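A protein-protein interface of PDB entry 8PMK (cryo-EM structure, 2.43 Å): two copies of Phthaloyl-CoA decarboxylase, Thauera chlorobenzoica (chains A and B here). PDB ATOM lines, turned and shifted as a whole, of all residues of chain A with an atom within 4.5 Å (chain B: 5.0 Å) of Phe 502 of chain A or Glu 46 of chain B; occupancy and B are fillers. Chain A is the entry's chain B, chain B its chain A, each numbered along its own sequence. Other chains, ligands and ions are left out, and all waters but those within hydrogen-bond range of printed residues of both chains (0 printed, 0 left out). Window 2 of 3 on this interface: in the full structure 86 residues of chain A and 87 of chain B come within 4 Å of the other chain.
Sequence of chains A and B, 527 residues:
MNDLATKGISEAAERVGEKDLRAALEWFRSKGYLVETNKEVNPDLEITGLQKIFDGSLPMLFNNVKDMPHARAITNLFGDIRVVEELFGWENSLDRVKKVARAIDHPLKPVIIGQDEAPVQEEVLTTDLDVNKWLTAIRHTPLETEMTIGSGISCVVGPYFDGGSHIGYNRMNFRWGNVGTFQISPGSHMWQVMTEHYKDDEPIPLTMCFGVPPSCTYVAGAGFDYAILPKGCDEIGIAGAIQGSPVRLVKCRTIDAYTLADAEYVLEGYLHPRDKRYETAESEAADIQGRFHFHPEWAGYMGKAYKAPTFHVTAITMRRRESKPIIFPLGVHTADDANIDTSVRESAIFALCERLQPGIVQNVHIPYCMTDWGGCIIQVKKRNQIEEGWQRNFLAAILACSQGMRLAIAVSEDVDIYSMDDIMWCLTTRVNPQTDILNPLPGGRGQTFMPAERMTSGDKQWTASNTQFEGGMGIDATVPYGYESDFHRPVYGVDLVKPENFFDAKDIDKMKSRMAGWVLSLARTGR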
ATOM      1  N   VAL A 497     -13.986   0.122 -18.968  1.00  0.00           N
ATOM      2  CA  VAL A 497     -15.232   0.858 -18.832  1.00  0.00           C
ATOM      3  C   VAL A 497     -14.899   2.236 -18.263  1.00  0.00           C
ATOM      4  O   VAL A 497     -13.868   2.430 -17.608  1.00  0.00           O
ATOM      5  CB  VAL A 497     -16.259   0.061 -17.970  1.00  0.00           C
ATOM      6  CG1 VAL A 497     -15.961   0.103 -16.469  1.00  0.00           C
ATOM      7  CG2 VAL A 497     -17.702   0.455 -18.276  1.00  0.00           C
ATOM      8  N   LYS A 498     -15.720   3.222 -18.616  1.00  0.00           N
ATOM      9  CA  LYS A 498     -15.575   4.577 -18.126  1.00  0.00           C
ATOM     10  C   LYS A 498     -16.832   4.972 -17.362  1.00  0.00           C
ATOM     11  O   LYS A 498     -17.939   4.843 -17.903  1.00  0.00           O
ATOM     12  CB  LYS A 498     -15.333   5.564 -19.277  1.00  0.00           C
ATOM     13  CG  LYS A 498     -14.196   5.178 -20.206  1.00  0.00           C
ATOM     14  CD  LYS A 498     -13.401   6.393 -20.643  1.00  0.00           C
ATOM     15  CE  LYS A 498     -14.245   7.326 -21.494  1.00  0.00           C
ATOM     16  NZ  LYS A 498     -14.913   6.602 -22.609  1.00  0.00           N
ATOM     17  N   PRO A 499     -16.715   5.455 -16.120  1.00  0.00           N
ATOM     18  CA  PRO A 499     -17.914   5.814 -15.351  1.00  0.00           C
ATOM     19  C   PRO A 499     -18.552   7.132 -15.755  1.00  0.00           C
ATOM     20  O   PRO A 499     -19.667   7.418 -15.300  1.00  0.00           O
ATOM     21  CB  PRO A 499     -17.396   5.888 -13.907  1.00  0.00           C
ATOM     22  CG  PRO A 499     -16.023   5.297 -13.935  1.00  0.00           C
ATOM     23  CD  PRO A 499     -15.502   5.565 -15.296  1.00  0.00           C
ATOM     24  N   GLU A 500     -17.891   7.940 -16.588  1.00  0.00           N
ATOM     25  CA  GLU A 500     -18.473   9.193 -17.050  1.00  0.00           C
ATOM     26  C   GLU A 500     -19.555   8.978 -18.099  1.00  0.00           C
ATOM     27  O   GLU A 500     -20.398   9.860 -18.291  1.00  0.00           O
ATOM     28  CB  GLU A 500     -17.385  10.102 -17.619  1.00  0.00           C
ATOM     29  CG  GLU A 500     -16.018   9.928 -16.973  1.00  0.00           C
ATOM     30  CD  GLU A 500     -15.986  10.402 -15.535  1.00  0.00           C
ATOM     31  OE1 GLU A 500     -16.584  11.459 -15.242  1.00  0.00           O
ATOM     32  OE2 GLU A 500     -15.363   9.716 -14.698  1.00  0.00           O
ATOM     33  N   ASN A 501     -19.555   7.830 -18.777  1.00  0.00           N
ATOM     34  CA  ASN A 501     -20.580   7.530 -19.765  1.00  0.00           C
ATOM     35  C   ASN A 501     -21.892   7.080 -19.140  1.00  0.00           C
ATOM     36  O   ASN A 501     -22.917   7.078 -19.827  1.00  0.00           O
ATOM     37  CB  ASN A 501     -20.088   6.447 -20.726  1.00  0.00           C
ATOM     38  CG  ASN A 501     -18.761   6.794 -21.364  1.00  0.00           C
ATOM     39  OD1 ASN A 501     -17.886   5.941 -21.500  1.00  0.00           O
ATOM     40  ND2 ASN A 501     -18.607   8.050 -21.766  1.00  0.00           N
ATOM     41  N   PHE A 502     -21.887   6.700 -17.866  1.00  0.00           N
ATOM     42  CA  PHE A 502     -23.071   6.174 -17.200  1.00  0.00           C
ATOM     43  C   PHE A 502     -23.686   7.134 -16.200  1.00  0.00           C
ATOM     44  O   PHE A 502     -24.911   7.201 -16.094  1.00  0.00           O
ATOM     45  CB  PHE A 502     -22.731   4.861 -16.492  1.00  0.00           C
ATOM     46  CG  PHE A 502     -22.432   3.738 -17.430  1.00  0.00           C
ATOM     47  CD1 PHE A 502     -23.472   2.999 -17.992  1.00  0.00           C
ATOM     48  CD2 PHE A 502     -21.113   3.427 -17.761  1.00  0.00           C
ATOM     49  CE1 PHE A 502     -23.205   1.957 -18.874  1.00  0.00           C
ATOM     50  CE2 PHE A 502     -20.832   2.386 -18.642  1.00  0.00           C
ATOM     51  CZ  PHE A 502     -21.881   1.650 -19.197  1.00  0.00           C
ATOM     52  N   PHE A 503     -22.874   7.881 -15.462  1.00  0.00           N
ATOM     53  CA  PHE A 503     -23.376   8.793 -14.450  1.00  0.00           C
ATOM     54  C   PHE A 503     -22.834  10.189 -14.701  1.00  0.00           C
ATOM     55  O   PHE A 503     -21.799  10.374 -15.344  1.00  0.00           O
ATOM     56  CB  PHE A 503     -22.989   8.342 -13.039  1.00  0.00           C
ATOM     57  CG  PHE A 503     -23.053   6.863 -12.842  1.00  0.00           C
ATOM     58  CD1 PHE A 503     -24.287   6.220 -12.745  1.00  0.00           C
ATOM     59  CD2 PHE A 503     -21.882   6.109 -12.759  1.00  0.00           C
ATOM     60  CE1 PHE A 503     -24.358   4.843 -12.561  1.00  0.00           C
ATOM     61  CE2 PHE A 503     -21.938   4.729 -12.577  1.00  0.00           C
ATOM     62  CZ  PHE A 503     -23.182   4.100 -12.481  1.00  0.00           C
ATOM     63  N   THR B  37     -29.222   4.954 -13.501  1.00  0.00           N
ATOM     64  CA  THR B  37     -28.842   5.358 -14.844  1.00  0.00           C
ATOM     65  C   THR B  37     -29.748   4.661 -15.843  1.00  0.00           C
ATOM     66  O   THR B  37     -30.390   3.655 -15.533  1.00  0.00           O
ATOM     67  CB  THR B  37     -27.384   5.026 -15.154  1.00  0.00           C
ATOM     68  OG1 THR B  37     -27.162   5.138 -16.564  1.00  0.00           O
ATOM     69  CG2 THR B  37     -27.077   3.621 -14.724  1.00  0.00           C
ATOM     70  N   LYS B  39     -28.414   4.324 -19.218  1.00  0.00           N
ATOM     71  CA  LYS B  39     -27.534   3.855 -20.273  1.00  0.00           C
ATOM     72  C   LYS B  39     -27.491   2.335 -20.279  1.00  0.00           C
ATOM     73  O   LYS B  39     -27.636   1.684 -19.240  1.00  0.00           O
ATOM     74  CB  LYS B  39     -26.126   4.413 -20.089  1.00  0.00           C
ATOM     75  CG  LYS B  39     -26.086   5.894 -19.785  1.00  0.00           C
ATOM     76  CD  LYS B  39     -26.580   6.712 -20.963  1.00  0.00           C
ATOM     77  CE  LYS B  39     -26.088   8.150 -20.891  1.00  0.00           C
ATOM     78  NZ  LYS B  39     -25.893   8.624 -19.491  1.00  0.00           N
ATOM     79  N   GLU B  40     -27.295   1.767 -21.463  1.00  0.00           N
ATOM     80  CA  GLU B  40     -27.325   0.316 -21.621  1.00  0.00           C
ATOM     81  C   GLU B  40     -25.986  -0.257 -21.185  1.00  0.00           C
ATOM     82  O   GLU B  40     -25.009  -0.230 -21.934  1.00  0.00           O
ATOM     83  CB  GLU B  40     -27.643  -0.070 -23.058  1.00  0.00           C
ATOM     84  CG  GLU B  40     -27.906  -1.549 -23.221  1.00  0.00           C
ATOM     85  CD  GLU B  40     -28.252  -1.934 -24.641  1.00  0.00           C
ATOM     86  OE1 GLU B  40     -27.322  -2.063 -25.464  1.00  0.00           O
ATOM     87  OE2 GLU B  40     -29.453  -2.112 -24.935  1.00  0.00           O
ATOM     88  N   VAL B  41     -25.940  -0.780 -19.964  1.00  0.00           N
ATOM     89  CA  VAL B  41     -24.746  -1.460 -19.487  1.00  0.00           C
ATOM     90  C   VAL B  41     -24.676  -2.856 -20.105  1.00  0.00           C
ATOM     91  O   VAL B  41     -25.671  -3.415 -20.577  1.00  0.00           O
ATOM     92  CB  VAL B  41     -24.719  -1.490 -17.938  1.00  0.00           C
ATOM     93  CG1 VAL B  41     -25.505  -2.654 -17.338  1.00  0.00           C
ATOM     94  CG2 VAL B  41     -23.289  -1.440 -17.383  1.00  0.00           C
ATOM     95  N   ASN B  42     -23.463  -3.382 -20.198  1.00  0.00           N
ATOM     96  CA  ASN B  42     -23.193  -4.719 -20.693  1.00  0.00           C
ATOM     97  C   ASN B  42     -23.087  -5.693 -19.531  1.00  0.00           C
ATOM     98  O   ASN B  42     -22.457  -5.377 -18.518  1.00  0.00           O
ATOM     99  CB  ASN B  42     -21.889  -4.741 -21.491  1.00  0.00           C
ATOM    100  CG  ASN B  42     -21.886  -5.780 -22.592  1.00  0.00           C
ATOM    101  OD1 ASN B  42     -22.237  -6.937 -22.376  1.00  0.00           O
ATOM    102  ND2 ASN B  42     -21.472  -5.370 -23.782  1.00  0.00           N
ATOM    103  N   PRO B  43     -23.708  -6.871 -19.617  1.00  0.00           N
ATOM    104  CA  PRO B  43     -23.384  -7.936 -18.653  1.00  0.00           C
ATOM    105  C   PRO B  43     -21.988  -8.512 -18.827  1.00  0.00           C
ATOM    106  O   PRO B  43     -21.439  -9.057 -17.863  1.00  0.00           O
ATOM    107  CB  PRO B  43     -24.463  -8.993 -18.917  1.00  0.00           C
ATOM    108  CG  PRO B  43     -25.018  -8.661 -20.260  1.00  0.00           C
ATOM    109  CD  PRO B  43     -24.926  -7.180 -20.381  1.00  0.00           C
ATOM    110  N   ASP B  44     -21.398  -8.411 -20.016  1.00  0.00           N
ATOM    111  CA  ASP B  44     -20.018  -8.819 -20.247  1.00  0.00           C
ATOM    112  C   ASP B  44     -19.100  -7.659 -19.885  1.00  0.00           C
ATOM    113  O   ASP B  44     -19.029  -6.666 -20.614  1.00  0.00           O
ATOM    114  CB  ASP B  44     -19.826  -9.243 -21.697  1.00  0.00           C
ATOM    115  CG  ASP B  44     -18.968 -10.481 -21.835  1.00  0.00           C
ATOM    116  OD1 ASP B  44     -17.857 -10.500 -21.272  1.00  0.00           O
ATOM    117  OD2 ASP B  44     -19.403 -11.437 -22.510  1.00  0.00           O
ATOM    118  N   LEU B  45     -18.436  -7.792 -18.722  1.00  0.00           N
ATOM    119  CA  LEU B  45     -17.277  -7.000 -18.264  1.00  0.00           C
ATOM    120  C   LEU B  45     -17.580  -5.515 -18.065  1.00  0.00           C
ATOM    121  O   LEU B  45     -16.691  -4.674 -18.214  1.00  0.00           O
ATOM    122  CB  LEU B  45     -16.069  -7.156 -19.197  1.00  0.00           C
ATOM    123  CG  LEU B  45     -15.612  -8.561 -19.581  1.00  0.00           C
ATOM    124  CD1 LEU B  45     -14.367  -8.493 -20.442  1.00  0.00           C
ATOM    125  CD2 LEU B  45     -15.375  -9.392 -18.346  1.00  0.00           C
ATOM    126  N   GLU B  46     -18.819  -5.166 -17.728  1.00  0.00           N
ATOM    127  CA  GLU B  46     -19.129  -3.763 -17.483  1.00  0.00           C
ATOM    128  C   GLU B  46     -19.882  -3.578 -16.175  1.00  0.00           C
ATOM    129  O   GLU B  46     -19.815  -2.505 -15.570  1.00  0.00           O
ATOM    130  CB  GLU B  46     -19.932  -3.175 -18.642  1.00  0.00           C
ATOM    131  CG  GLU B  46     -19.093  -2.730 -19.823  1.00  0.00           C
ATOM    132  CD  GLU B  46     -19.863  -1.843 -20.779  1.00  0.00           C
ATOM    133  OE1 GLU B  46     -21.009  -1.469 -20.454  1.00  0.00           O
ATOM    134  OE2 GLU B  46     -19.323  -1.517 -21.856  1.00  0.00           O
ATOM    135  N   ILE B  47     -20.609  -4.603 -15.739  1.00  0.00           N
ATOM    136  CA  ILE B  47     -21.280  -4.536 -14.446  1.00  0.00           C
ATOM    137  C   ILE B  47     -20.272  -4.706 -13.319  1.00  0.00           C
ATOM    138  O   ILE B  47     -20.195  -3.879 -12.403  1.00  0.00           O
ATOM    139  CB  ILE B  47     -22.406  -5.585 -14.378  1.00  0.00           C
ATOM    140  CG1 ILE B  47     -23.544  -5.186 -15.312  1.00  0.00           C
ATOM    141  CG2 ILE B  47     -22.942  -5.737 -12.963  1.00  0.00           C
ATOM    142  CD1 ILE B  47     -24.633  -6.223 -15.440  1.00  0.00           C
ATOM    143  N   THR B  48     -19.454  -5.752 -13.398  1.00  0.00           N
ATOM    144  CA  THR B  48     -18.413  -5.979 -12.408  1.00  0.00           C
ATOM    145  C   THR B  48     -17.223  -5.048 -12.575  1.00  0.00           C
ATOM    146  O   THR B  48     -16.454  -4.881 -11.623  1.00  0.00           O
ATOM    147  CB  THR B  48     -17.933  -7.422 -12.481  1.00  0.00           C
ATOM    148  OG1 THR B  48     -17.509  -7.703 -13.818  1.00  0.00           O
ATOM    149  CG2 THR B  48     -19.059  -8.357 -12.114  1.00  0.00           C
ATOM    150  N   GLY B  49     -17.035  -4.479 -13.768  1.00  0.00           N
ATOM    151  CA  GLY B  49     -16.030  -3.443 -13.936  1.00  0.00           C
ATOM    152  C   GLY B  49     -16.402  -2.154 -13.230  1.00  0.00           C
ATOM    153  O   GLY B  49     -15.562  -1.532 -12.578  1.00  0.00           O
ATOM    154  N   LEU B  50     -17.670  -1.754 -13.323  1.00  0.00           N
ATOM    155  CA  LEU B  50     -18.154  -0.587 -12.599  1.00  0.00           C
ATOM    156  C   LEU B  50     -18.330  -0.856 -11.114  1.00  0.00           C
ATOM    157  O   LEU B  50     -18.329   0.089 -10.322  1.00  0.00           O
ATOM    158  CB  LEU B  50     -19.482  -0.114 -13.187  1.00  0.00           C
ATOM    159  CG  LEU B  50     -19.394   0.708 -14.468  1.00  0.00           C
ATOM    160  CD1 LEU B  50     -20.742   0.761 -15.149  1.00  0.00           C
ATOM    161  CD2 LEU B  50     -18.897   2.101 -14.160  1.00  0.00           C
ATOM    162  N   PHE B  62     -29.038  -0.281 -12.621  1.00  0.00           N
ATOM    163  CA  PHE B  62     -28.963  -0.258 -14.076  1.00  0.00           C
ATOM    164  C   PHE B  62     -30.336  -0.606 -14.626  1.00  0.00           C
ATOM    165  O   PHE B  62     -30.793  -1.745 -14.491  1.00  0.00           O
ATOM    166  CB  PHE B  62     -27.913  -1.238 -14.581  1.00  0.00           C
ATOM    167  CG  PHE B  62     -26.520  -0.880 -14.186  1.00  0.00           C
ATOM    168  CD1 PHE B  62     -25.856   0.159 -14.831  1.00  0.00           C
ATOM    169  CD2 PHE B  62     -25.875  -1.576 -13.163  1.00  0.00           C
ATOM    170  CE1 PHE B  62     -24.558   0.505 -14.469  1.00  0.00           C
ATOM    171  CE2 PHE B  62     -24.577  -1.242 -12.791  1.00  0.00           C
ATOM    172  CZ  PHE B  62     -23.922  -0.199 -13.447  1.00  0.00           C
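The backbone carbonyl oxygen (O) of Phe 502 of chain A is in hydrogen-bond range of the side-chain hydroxyl (OG1) of Thr 37 of chain B (3.1 Å). The side-chain amino group of Lys 39 of chain B is in hydrogen-bond range of the backbone carbonyl oxygen of Asn 501 of chain A, at 3.4 Å.
No position is printed for both chains. Of the 9 pairs that touch across the chains among the printed residues, none has its exchanged pair printed and touching as well.
The side-chain hydroxyl (OG1) of Thr 37 of chain B sits at hydrogen-bond distance from the backbone NH (N) of Lys 39 of chain B (3.0 Å). N of Asn 42 of chain B lies within hydrogen-bond range of OE1 of Glu 46 of chain B, 3.1 Å away. The side-chain amino group of Lys 498 of chain A is in hydrogen-bond range of the side-chain amide oxygen of Asn 501 of chain A, at 3.2 Å.
Among the printed residues, pairs that only touch across the chains: Phe 502 of chain A with Glu 46 of chain B, Phe 502 of chain A with Lys 39 of chain B, Phe 503 of chain A with Thr 37 of chain B, Phe 502 of chain A with Val 41 of chain B, Phe 502 of chain A with Leu 50 of chain B, Val 497 of chain A with Glu 46 of chain B and Val 497 of chain A with Gly 49 of chain B.
Hydrophobic or aromatic side chains of chain B that line the printed part of chain A: Val 41 and Leu 50. Along chain B the printed residues that touch a printed residue of chain A span positions 37 to 50. Hydrophobic or aromatic side chains of chain A within 4 Å of the printed part of chain B: Val 497, Phe 502 and Phe 503. Among the printed residues, no Asp or Glu carboxylate lies within 4 Å of a Lys or Arg side-chain nitrogen of the other chain.
Of the printed residues of chain B, Asn 501 of chain A touches Lys 39 (3.4 Å). Phe 502 of chain A touches just these residues of chain B: Thr 37 (3.1 Å), Lys 39 (3.7 Å), Val 41 (3.7 Å), Glu 46 (3.5 Å) and Leu 50 (3.8 Å). Printed residues of chain B within 4 Å of Phe 503 of chain A: Thr 37 (3.7 Å). Of the printed residues of chain A, Thr 37 of chain B touches Phe 502 and Phe 503. Printed residues of chain A within 4 Å of Lys 39 of chain B: Asn 501 (3.4 Å) and Phe 502 (3.7 Å). Printed residues of chain A within 4 Å of Val 41 of chain B: Phe 502. Of chain A, only Val 497 and Phe 502 come within 4 Å of Glu 46 of chain B. The nearest printed residue of chain A that does not touch Thr 37 of chain B is Asn 501 of chain A (5.7 Å).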
